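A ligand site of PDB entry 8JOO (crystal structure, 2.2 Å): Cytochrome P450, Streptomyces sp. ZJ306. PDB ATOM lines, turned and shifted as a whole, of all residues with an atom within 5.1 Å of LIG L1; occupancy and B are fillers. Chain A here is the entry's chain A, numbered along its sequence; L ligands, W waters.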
ATOM      1  N   ARG A  86     -16.464   0.083   6.386  1.00  0.00           N
ATOM      2  CA  ARG A  86     -15.702  -1.049   5.907  1.00  0.00           C
ATOM      3  C   ARG A  86     -14.765  -1.556   6.992  1.00  0.00           C
ATOM      4  O   ARG A  86     -14.177  -0.766   7.736  1.00  0.00           O
ATOM      5  CB  ARG A  86     -14.896  -0.674   4.658  1.00  0.00           C
ATOM      6  CG  ARG A  86     -14.450  -1.900   3.853  1.00  0.00           C
ATOM      7  CD  ARG A  86     -13.591  -1.506   2.672  1.00  0.00           C
ATOM      8  NE  ARG A  86     -12.308  -0.945   3.055  1.00  0.00           N
ATOM      9  CZ  ARG A  86     -11.537  -0.208   2.249  1.00  0.00           C
ATOM     10  NH1 ARG A  86     -11.906   0.065   1.006  1.00  0.00           N
ATOM     11  NH2 ARG A  86     -10.384   0.247   2.705  1.00  0.00           N
ATOM     12  N   ALA A  89      -9.564  -0.300   7.297  1.00  0.00           N
ATOM     13  CA  ALA A  89      -9.549   1.139   7.077  1.00  0.00           C
ATOM     14  C   ALA A  89      -8.991   1.469   5.696  1.00  0.00           C
ATOM     15  O   ALA A  89      -8.172   0.726   5.139  1.00  0.00           O
ATOM     16  CB  ALA A  89      -8.727   1.845   8.159  1.00  0.00           C
ATOM     17  N   ARG A  90      -9.422   2.607   5.141  1.00  0.00           N
ATOM     18  CA  ARG A  90      -9.085   3.002   3.774  1.00  0.00           C
ATOM     19  C   ARG A  90      -7.778   3.780   3.789  1.00  0.00           C
ATOM     20  O   ARG A  90      -7.752   5.001   3.958  1.00  0.00           O
ATOM     21  CB  ARG A  90     -10.215   3.836   3.175  1.00  0.00           C
ATOM     22  CG  ARG A  90     -11.621   3.351   3.459  1.00  0.00           C
ATOM     23  CD  ARG A  90     -12.615   4.182   2.662  1.00  0.00           C
ATOM     24  NE  ARG A  90     -14.005   3.826   2.906  1.00  0.00           N
ATOM     25  CZ  ARG A  90     -14.645   2.858   2.275  1.00  0.00           C
ATOM     26  NH1 ARG A  90     -14.051   2.109   1.364  1.00  0.00           N
ATOM     27  NH2 ARG A  90     -15.922   2.621   2.587  1.00  0.00           N
ATOM     28  N   VAL A  91      -6.666   3.082   3.558  1.00  0.00           N
ATOM     29  CA  VAL A  91      -5.337   3.680   3.626  1.00  0.00           C
ATOM     30  C   VAL A  91      -4.527   3.244   2.419  1.00  0.00           C
ATOM     31  O   VAL A  91      -4.588   2.083   1.990  1.00  0.00           O
ATOM     32  CB  VAL A  91      -4.612   3.329   4.940  1.00  0.00           C
ATOM     33  CG1 VAL A  91      -5.518   3.597   6.125  1.00  0.00           C
ATOM     34  CG2 VAL A  91      -4.167   1.878   4.918  1.00  0.00           C
ATOM     35  N   GLY A  92      -3.763   4.183   1.876  1.00  0.00           N
ATOM     36  CA  GLY A  92      -2.940   3.907   0.710  1.00  0.00           C
ATOM     37  C   GLY A  92      -2.025   5.084   0.422  1.00  0.00           C
ATOM     38  O   GLY A  92      -1.785   5.923   1.289  1.00  0.00           O
ATOM     39  N   PHE A  96      -6.563  10.233  -1.960  1.00  0.00           N
ATOM     40  CA  PHE A  96      -7.392  10.260  -0.756  1.00  0.00           C
ATOM     41  C   PHE A  96      -6.581  10.137   0.525  1.00  0.00           C
ATOM     42  O   PHE A  96      -7.167  10.226   1.608  1.00  0.00           O
ATOM     43  CB  PHE A  96      -8.437   9.124  -0.823  1.00  0.00           C
ATOM     44  CG  PHE A  96      -9.689   9.471  -1.583  1.00  0.00           C
ATOM     45  CD1 PHE A  96     -10.477  10.562  -1.215  1.00  0.00           C
ATOM     46  CD2 PHE A  96     -10.096   8.685  -2.651  1.00  0.00           C
ATOM     47  CE1 PHE A  96     -11.624  10.886  -1.897  1.00  0.00           C
ATOM     48  CE2 PHE A  96     -11.261   9.000  -3.343  1.00  0.00           C
ATOM     49  CZ  PHE A  96     -12.019  10.090  -2.968  1.00  0.00           C
ATOM     50  N   ILE A 180     -12.931  -2.862  -3.077  1.00  0.00           N
ATOM     51  CA  ILE A 180     -12.669  -1.585  -2.418  1.00  0.00           C
ATOM     52  C   ILE A 180     -13.950  -1.021  -1.829  1.00  0.00           C
ATOM     53  O   ILE A 180     -13.940  -0.435  -0.736  1.00  0.00           O
ATOM     54  CB  ILE A 180     -12.013  -0.596  -3.408  1.00  0.00           C
ATOM     55  CG1 ILE A 180     -10.530  -0.913  -3.615  1.00  0.00           C
ATOM     56  CG2 ILE A 180     -12.226   0.852  -2.946  1.00  0.00           C
ATOM     57  CD1 ILE A 180      -9.703  -0.736  -2.389  1.00  0.00           C
ATOM     58  N   LEU A 181     -15.068  -1.197  -2.518  1.00  0.00           N
ATOM     59  CA  LEU A 181     -16.322  -0.565  -2.138  1.00  0.00           C
ATOM     60  C   LEU A 181     -17.216  -1.469  -1.312  1.00  0.00           C
ATOM     61  O   LEU A 181     -18.261  -1.011  -0.820  1.00  0.00           O
ATOM     62  CB  LEU A 181     -17.054  -0.103  -3.400  1.00  0.00           C
ATOM     63  CG  LEU A 181     -16.255   0.944  -4.183  1.00  0.00           C
ATOM     64  CD1 LEU A 181     -16.504   0.882  -5.686  1.00  0.00           C
ATOM     65  CD2 LEU A 181     -16.537   2.344  -3.633  1.00  0.00           C
ATOM     66  N   LEU A 190      -8.010  -6.662   0.995  1.00  0.00           N
ATOM     67  CA  LEU A 190      -7.314  -5.511   0.453  1.00  0.00           C
ATOM     68  C   LEU A 190      -5.865  -5.848   0.131  1.00  0.00           C
ATOM     69  O   LEU A 190      -5.299  -5.366  -0.846  1.00  0.00           O
ATOM     70  CB  LEU A 190      -7.379  -4.344   1.440  1.00  0.00           C
ATOM     71  CG  LEU A 190      -8.763  -3.888   1.907  1.00  0.00           C
ATOM     72  CD1 LEU A 190      -8.682  -3.332   3.317  1.00  0.00           C
ATOM     73  CD2 LEU A 190      -9.309  -2.849   0.951  1.00  0.00           C
ATOM     74  N   ARG A 193      -6.199  -7.827  -3.159  1.00  0.00           N
ATOM     75  CA  ARG A 193      -6.412  -6.877  -4.234  1.00  0.00           C
ATOM     76  C   ARG A 193      -5.099  -6.170  -4.568  1.00  0.00           C
ATOM     77  O   ARG A 193      -4.673  -6.127  -5.731  1.00  0.00           O
ATOM     78  CB  ARG A 193      -7.470  -5.829  -3.870  1.00  0.00           C
ATOM     79  CG  ARG A 193      -7.594  -4.762  -4.950  1.00  0.00           C
ATOM     80  CD  ARG A 193      -8.344  -3.501  -4.526  1.00  0.00           C
ATOM     81  NE  ARG A 193      -8.146  -2.430  -5.499  1.00  0.00           N
ATOM     82  CZ  ARG A 193      -7.028  -1.728  -5.636  1.00  0.00           C
ATOM     83  NH1 ARG A 193      -5.988  -1.929  -4.836  1.00  0.00           N
ATOM     84  NH2 ARG A 193      -6.947  -0.814  -6.597  1.00  0.00           N
ATOM     85  N   SER A 240      -4.298   3.337  -9.670  1.00  0.00           N
ATOM     86  CA  SER A 240      -5.278   2.655  -8.832  1.00  0.00           C
ATOM     87  C   SER A 240      -6.447   3.565  -8.522  1.00  0.00           C
ATOM     88  O   SER A 240      -7.611   3.133  -8.584  1.00  0.00           O
ATOM     89  CB  SER A 240      -4.618   2.165  -7.532  1.00  0.00           C
ATOM     90  OG  SER A 240      -5.434   1.218  -6.868  1.00  0.00           O
ATOM     91  N   ASP A 241      -6.175   4.830  -8.199  1.00  0.00           N
ATOM     92  CA  ASP A 241      -7.243   5.768  -7.898  1.00  0.00           C
ATOM     93  C   ASP A 241      -8.222   5.886  -9.060  1.00  0.00           C
ATOM     94  O   ASP A 241      -9.442   5.836  -8.870  1.00  0.00           O
ATOM     95  CB  ASP A 241      -6.676   7.156  -7.569  1.00  0.00           C
ATOM     96  CG  ASP A 241      -6.116   7.250  -6.167  1.00  0.00           C
ATOM     97  OD1 ASP A 241      -6.458   6.412  -5.313  1.00  0.00           O
ATOM     98  OD2 ASP A 241      -5.318   8.172  -5.920  1.00  0.00           O
ATOM     99  N   SER A 244     -10.150   2.677  -9.842  1.00  0.00           N
ATOM    100  CA  SER A 244     -11.032   2.304  -8.735  1.00  0.00           C
ATOM    101  C   SER A 244     -12.225   3.244  -8.630  1.00  0.00           C
ATOM    102  O   SER A 244     -13.352   2.782  -8.432  1.00  0.00           O
ATOM    103  CB  SER A 244     -10.279   2.293  -7.398  1.00  0.00           C
ATOM    104  OG  SER A 244     -10.968   1.524  -6.422  1.00  0.00           O
ATOM    105  N   ALA A 245     -11.996   4.548  -8.761  1.00  0.00           N
ATOM    106  CA  ALA A 245     -13.037   5.554  -8.633  1.00  0.00           C
ATOM    107  C   ALA A 245     -13.660   5.933  -9.978  1.00  0.00           C
ATOM    108  O   ALA A 245     -14.596   6.725 -10.004  1.00  0.00           O
ATOM    109  CB  ALA A 245     -12.475   6.825  -7.963  1.00  0.00           C
ATOM    110  N   SER A 249     -19.010   4.291 -10.039  1.00  0.00           N
ATOM    111  CA  SER A 249     -19.990   5.297  -9.612  1.00  0.00           C
ATOM    112  C   SER A 249     -20.839   5.762 -10.783  1.00  0.00           C
ATOM    113  O   SER A 249     -22.071   5.903 -10.662  1.00  0.00           O
ATOM    114  CB  SER A 249     -19.282   6.494  -8.990  1.00  0.00           C
ATOM    115  OG  SER A 249     -18.197   6.072  -8.192  1.00  0.00           O
ATOM    116  N   ILE A 291     -26.624   8.819  -3.673  1.00  0.00           N
ATOM    117  CA  ILE A 291     -25.878   7.718  -4.256  1.00  0.00           C
ATOM    118  C   ILE A 291     -25.333   6.800  -3.162  1.00  0.00           C
ATOM    119  O   ILE A 291     -25.226   5.586  -3.353  1.00  0.00           O
ATOM    120  CB  ILE A 291     -24.751   8.246  -5.165  1.00  0.00           C
ATOM    121  CG1 ILE A 291     -23.922   7.093  -5.730  1.00  0.00           C
ATOM    122  CG2 ILE A 291     -23.845   9.209  -4.413  1.00  0.00           C
ATOM    123  CD1 ILE A 291     -24.562   6.332  -6.862  1.00  0.00           C
ATOM    124  N   LEU A 292     -24.979   7.368  -2.017  1.00  0.00           N
ATOM    125  CA  LEU A 292     -24.266   6.605  -0.997  1.00  0.00           C
ATOM    126  C   LEU A 292     -25.212   6.064   0.073  1.00  0.00           C
ATOM    127  O   LEU A 292     -26.089   6.778   0.570  1.00  0.00           O
ATOM    128  CB  LEU A 292     -23.179   7.453  -0.330  1.00  0.00           C
ATOM    129  CG  LEU A 292     -21.931   7.718  -1.158  1.00  0.00           C
ATOM    130  CD1 LEU A 292     -20.880   8.358  -0.272  1.00  0.00           C
ATOM    131  CD2 LEU A 292     -21.385   6.452  -1.804  1.00  0.00           C
ATOM    132  N   SER A 296     -18.232   8.969   2.694  1.00  0.00           N
ATOM    133  CA  SER A 296     -16.913   8.964   2.082  1.00  0.00           C
ATOM    134  C   SER A 296     -15.815   9.023   3.138  1.00  0.00           C
ATOM    135  O   SER A 296     -15.878   8.339   4.152  1.00  0.00           O
ATOM    136  CB  SER A 296     -16.815  10.147   1.103  1.00  0.00           C
ATOM    137  OG  SER A 296     -15.685  10.065   0.244  1.00  0.00           O
ATOM    138  N   PHE A 297     -14.792   9.807   2.891  1.00  0.00           N
ATOM    139  CA  PHE A 297     -13.729   9.887   3.890  1.00  0.00           C
ATOM    140  C   PHE A 297     -14.107  10.882   4.991  1.00  0.00           C
ATOM    141  O   PHE A 297     -14.596  11.972   4.696  1.00  0.00           O
ATOM    142  CB  PHE A 297     -12.410  10.291   3.234  1.00  0.00           C
ATOM    143  CG  PHE A 297     -11.769   9.162   2.479  1.00  0.00           C
ATOM    144  CD1 PHE A 297     -12.173   8.875   1.179  1.00  0.00           C
ATOM    145  CD2 PHE A 297     -10.779   8.391   3.059  1.00  0.00           C
ATOM    146  CE1 PHE A 297     -11.593   7.817   0.466  1.00  0.00           C
ATOM    147  CE2 PHE A 297     -10.190   7.332   2.352  1.00  0.00           C
ATOM    148  CZ  PHE A 297     -10.600   7.056   1.060  1.00  0.00           C
ATOM    149  N   ILE A 322     -22.803  14.217   1.907  1.00  0.00           N
ATOM    150  CA  ILE A 322     -23.150  14.889   0.659  1.00  0.00           C
ATOM    151  C   ILE A 322     -24.651  14.835   0.413  1.00  0.00           C
ATOM    152  O   ILE A 322     -25.258  15.807  -0.036  1.00  0.00           O
ATOM    153  CB  ILE A 322     -22.332  14.274  -0.491  1.00  0.00           C
ATOM    154  CG1 ILE A 322     -20.921  14.910  -0.514  1.00  0.00           C
ATOM    155  CG2 ILE A 322     -23.045  14.464  -1.830  1.00  0.00           C
ATOM    156  CD1 ILE A 322     -19.898  14.101  -1.284  1.00  0.00           C
ATOM    157  N   PHE A 397     -22.551  -0.303  -0.084  1.00  0.00           N
ATOM    158  CA  PHE A 397     -21.928   1.013   0.115  1.00  0.00           C
ATOM    159  C   PHE A 397     -22.589   2.065  -0.771  1.00  0.00           C
ATOM    160  O   PHE A 397     -22.897   3.165  -0.302  1.00  0.00           O
ATOM    161  CB  PHE A 397     -20.425   0.915  -0.154  1.00  0.00           C
ATOM    162  CG  PHE A 397     -19.678   2.218   0.018  1.00  0.00           C
ATOM    163  CD1 PHE A 397     -19.529   2.781   1.282  1.00  0.00           C
ATOM    164  CD2 PHE A 397     -19.133   2.860  -1.070  1.00  0.00           C
ATOM    165  CE1 PHE A 397     -18.843   3.976   1.453  1.00  0.00           C
ATOM    166  CE2 PHE A 397     -18.442   4.064  -0.908  1.00  0.00           C
ATOM    167  CZ  PHE A 397     -18.301   4.617   0.351  1.00  0.00           C
ATOM    168  N   MET A 398     -22.813   1.743  -2.040  1.00  0.00           N
ATOM    169  CA  MET A 398     -23.538   2.607  -2.963  1.00  0.00           C
ATOM    170  C   MET A 398     -24.957   2.080  -3.148  1.00  0.00           C
ATOM    171  O   MET A 398     -25.197   0.865  -3.144  1.00  0.00           O
ATOM    172  CB  MET A 398     -22.845   2.663  -4.324  1.00  0.00           C
ATOM    173  CG  MET A 398     -21.543   3.401  -4.358  1.00  0.00           C
ATOM    174  SD  MET A 398     -21.087   3.752  -6.064  1.00  0.00           S
ATOM    175  CE  MET A 398     -19.539   4.626  -5.829  1.00  0.00           C
HETATM  176  C1  LIG L   1     -14.265   5.969  -1.922  1.00  0.00           C
HETATM  177  C2  LIG L   1     -18.806   8.581  -5.472  1.00  0.00           C
HETATM  178  C3  LIG L   1     -12.183   4.384  -4.680  1.00  0.00           C
HETATM  179  C4  LIG L   1      -9.833   5.286  -4.815  1.00  0.00           C
HETATM  180  C5  LIG L   1     -11.139   5.438  -4.895  1.00  0.00           C
HETATM  181  C6  LIG L   1      -6.027   3.371  -3.302  1.00  0.00           C
HETATM  182  C7  LIG L   1     -11.007   4.322  -1.351  1.00  0.00           C
HETATM  183  C8  LIG L   1     -13.347   4.896  -3.828  1.00  0.00           C
HETATM  184  C9  LIG L   1     -12.301   4.412  -1.564  1.00  0.00           C
HETATM  185  C10 LIG L   1      -9.131   4.000  -4.583  1.00  0.00           C
HETATM  186  C11 LIG L   1      -6.884   2.936  -4.471  1.00  0.00           C
HETATM  187  C12 LIG L   1      -6.183   2.612  -1.991  1.00  0.00           C
HETATM  188  C13 LIG L   1     -10.337   3.350  -0.531  1.00  0.00           C
HETATM  189  C14 LIG L   1      -8.300   2.255   0.383  1.00  0.00           C
HETATM  190  C15 LIG L   1      -9.002   3.258  -0.422  1.00  0.00           C
HETATM  191  C16 LIG L   1      -6.676   3.460  -0.805  1.00  0.00           C
HETATM  192  N1  LIG L   1      -7.773   4.027  -4.674  1.00  0.00           N
HETATM  193  C17 LIG L   1     -18.178   7.691  -4.396  1.00  0.00           C
HETATM  194  C18 LIG L   1     -12.923   5.443  -2.437  1.00  0.00           C
HETATM  195  C19 LIG L   1     -20.188   8.152  -5.919  1.00  0.00           C
HETATM  196  C20 LIG L   1     -18.463   9.796  -2.917  1.00  0.00           C
HETATM  197  C21 LIG L   1     -18.241   8.290  -2.982  1.00  0.00           C
HETATM  198  C22 LIG L   1     -16.915   7.881  -2.305  1.00  0.00           C
HETATM  199  C23 LIG L   1      -8.027   4.142  -0.984  1.00  0.00           C
HETATM  200  C24 LIG L   1     -16.227   6.880  -3.223  1.00  0.00           C
HETATM  201  C25 LIG L   1     -16.669   7.434  -4.587  1.00  0.00           C
HETATM  202  C26 LIG L   1     -14.706   6.803  -3.127  1.00  0.00           C
HETATM  203  C27 LIG L   1     -14.075   6.141  -4.394  1.00  0.00           C
HETATM  204  C28 LIG L   1     -15.023   5.948  -5.542  1.00  0.00           C
HETATM  205  C29 LIG L   1     -16.209   6.526  -5.686  1.00  0.00           C
HETATM  206  N2  LIG L   1      -6.988   2.452   0.201  1.00  0.00           N
HETATM  207  O1  LIG L   1      -9.705   2.955  -4.344  1.00  0.00           O
HETATM  208  O2  LIG L   1     -11.119   2.472   0.117  1.00  0.00           O
HETATM  209  O3  LIG L   1      -8.802   1.350   1.055  1.00  0.00           O
HETATM  210  O4  LIG L   1      -8.142   5.263  -1.458  1.00  0.00           O
HETATM  211  C1  LG2 L   2     -13.475  11.931  -5.812  1.00  0.00           C
HETATM  212  C2  LG2 L   2     -18.213  11.690  -6.910  1.00  0.00           C
HETATM  213  C3  LG2 L   2     -17.180   9.922 -11.294  1.00  0.00           C
HETATM  214  C4  LG2 L   2     -12.470   9.824 -10.124  1.00  0.00           C
HETATM  215  C5  LG2 L   2     -14.859  12.095  -5.729  1.00  0.00           C
HETATM  216  C6  LG2 L   2     -15.617  12.749  -4.672  1.00  0.00           C
HETATM  217  C7  LG2 L   2     -16.904  12.669  -4.996  1.00  0.00           C
HETATM  218  C8  LG2 L   2     -17.021  11.965  -6.260  1.00  0.00           C
HETATM  219  C9  LG2 L   2     -18.100  13.212  -4.187  1.00  0.00           C
HETATM  220  C10 LG2 L   2     -15.030  13.402  -3.406  1.00  0.00           C
HETATM  221  C11 LG2 L   2     -15.259  12.503  -2.208  1.00  0.00           C
HETATM  222  C12 LG2 L   2     -14.685  13.116  -0.961  1.00  0.00           C
HETATM  223  O1  LG2 L   2     -14.091  14.221  -1.059  1.00  0.00           O
HETATM  224  O2  LG2 L   2     -14.821  12.495   0.136  1.00  0.00           O
HETATM  225  C13 LG2 L   2     -18.323  11.156  -8.162  1.00  0.00           C
HETATM  226  C14 LG2 L   2     -19.561  10.803  -8.816  1.00  0.00           C
HETATM  227  C15 LG2 L   2     -19.260  10.319 -10.023  1.00  0.00           C
HETATM  228  C16 LG2 L   2     -17.834  10.354 -10.166  1.00  0.00           C
HETATM  229  C17 LG2 L   2     -20.950  10.980  -8.181  1.00  0.00           C
HETATM  230  C18 LG2 L   2     -20.187   9.806 -11.140  1.00  0.00           C
HETATM  231  C19 LG2 L   2     -21.481  10.147 -11.157  1.00  0.00           C
HETATM  232  C20 LG2 L   2     -15.811   9.819 -11.387  1.00  0.00           C
HETATM  233  C21 LG2 L   2     -15.076   9.595 -12.599  1.00  0.00           C
HETATM  234  C22 LG2 L   2     -13.784   9.585 -12.305  1.00  0.00           C
HETATM  235  C23 LG2 L   2     -13.642   9.769 -10.872  1.00  0.00           C
HETATM  236  C24 LG2 L   2     -15.711   9.443 -13.999  1.00  0.00           C
HETATM  237  C25 LG2 L   2     -12.676   9.373 -13.340  1.00  0.00           C
HETATM  238  C26 LG2 L   2     -11.476   9.875 -13.127  1.00  0.00           C
HETATM  239  C27 LG2 L   2     -12.326  10.388  -8.851  1.00  0.00           C
HETATM  240  C28 LG2 L   2     -11.084  10.521  -8.096  1.00  0.00           C
HETATM  241  C29 LG2 L   2     -11.354  11.074  -6.918  1.00  0.00           C
HETATM  242  C30 LG2 L   2     -12.787  11.339  -6.868  1.00  0.00           C
HETATM  243  C31 LG2 L   2      -9.701  10.075  -8.599  1.00  0.00           C
HETATM  244  C32 LG2 L   2     -10.345  11.416  -5.806  1.00  0.00           C
HETATM  245  C33 LG2 L   2      -9.792  12.801  -6.112  1.00  0.00           C
HETATM  246  C34 LG2 L   2      -8.966  13.397  -5.002  1.00  0.00           C
HETATM  247  O3  LG2 L   2      -8.260  14.409  -5.263  1.00  0.00           O
HETATM  248  O4  LG2 L   2      -9.001  12.833  -3.877  1.00  0.00           O
HETATM  249  N1  LG2 L   2     -15.750  11.622  -6.694  1.00  0.00           N
HETATM  250  N2  LG2 L   2     -17.275  10.867  -9.009  1.00  0.00           N
HETATM  251  N3  LG2 L   2     -14.913   9.922 -10.352  1.00  0.00           N
HETATM  252  N4  LG2 L   2     -13.345  10.896  -8.061  1.00  0.00           N
HETATM  253 FE1  LG2 L   2     -15.285  10.981  -8.599  1.00  0.00          FE
HETATM  254  O   HOH W   1      -3.971   4.954  -4.806  1.00  0.00           O
HETATM  255  O   HOH W   2      -6.498   7.267  -2.744  1.00  0.00           O
HETATM  256  O   HOH W   3     -15.465   8.948  -7.949  1.00  0.00           O
HETATM  257  O   HOH W   4      -2.656   3.683  -2.770  1.00  0.00           O
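Water W2 lies within hydrogen-bond range of OD1 of Asp 241 (2.7 Å), O4 of LIG L1 (2.9 Å) and N of Phe 96 (3.1 Å).
The backbone carbonyl oxygen of Ile 180 is in hydrogen-bond range of the guanidinium group of Arg 86 (2.7 Å).
The backbone carbonyl oxygen (O) of Ala 89 sits at hydrogen-bond distance from the guanidinium group (NH2) of Arg 86.
NH1 of Arg 90 lies within hydrogen-bond range of O of Ile 180.
OG of Ser 240 sits at hydrogen-bond distance from NH2 of Arg 193 (2.5 Å).
CE2 of Phe 96 touches C5 of LIG L1 (3.9 Å).
Ile 180 touches LIG L1.
Ser 240 touches LIG L1.
Ala 245 touches LIG L1.
Ser 249 touches LIG L1 (OG to C29, 3.2 Å).
Ile 291 touches LIG L1 (CG1 to C19, 3.9 Å).
CD1 of Leu 292 touches C21 of LIG L1, 3.8 Å away.
Ser 296 touches LIG L1 (OG to C22, 3.6 Å).
Phe 297 touches LIG L1.
Met 398 touches LIG L1.
Hydrophobic or aromatic side chains that line LIG L1: Phe 96, Ile 180, Ala 245, Ile 291, Leu 292, Phe 297 and Met 398.
Of the 22 residues printed, 15 come within 4 Å of LIG L1.
The guanidinium group (NH2) of Arg 86 sits at hydrogen-bond distance from an oxygen (O3) of LIG L1 (2.5 Å).
The side-chain carboxylate of Asp 241 lies within hydrogen-bond range of a nitrogen (N1) of LIG L1 (2.8 Å).
O1 of LIG L1 lies within hydrogen-bond range of OG of Ser 244 (2.8 Å).
O of Val 91 lies within hydrogen-bond range of N2 of LIG L1 (3.0 Å).
The guanidinium group of Arg 90 lies within hydrogen-bond range of an oxygen (O2) of LIG L1, at 3.2 Å.
OG of Ser 296 is in hydrogen-bond range of O2 of LG2 L2.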
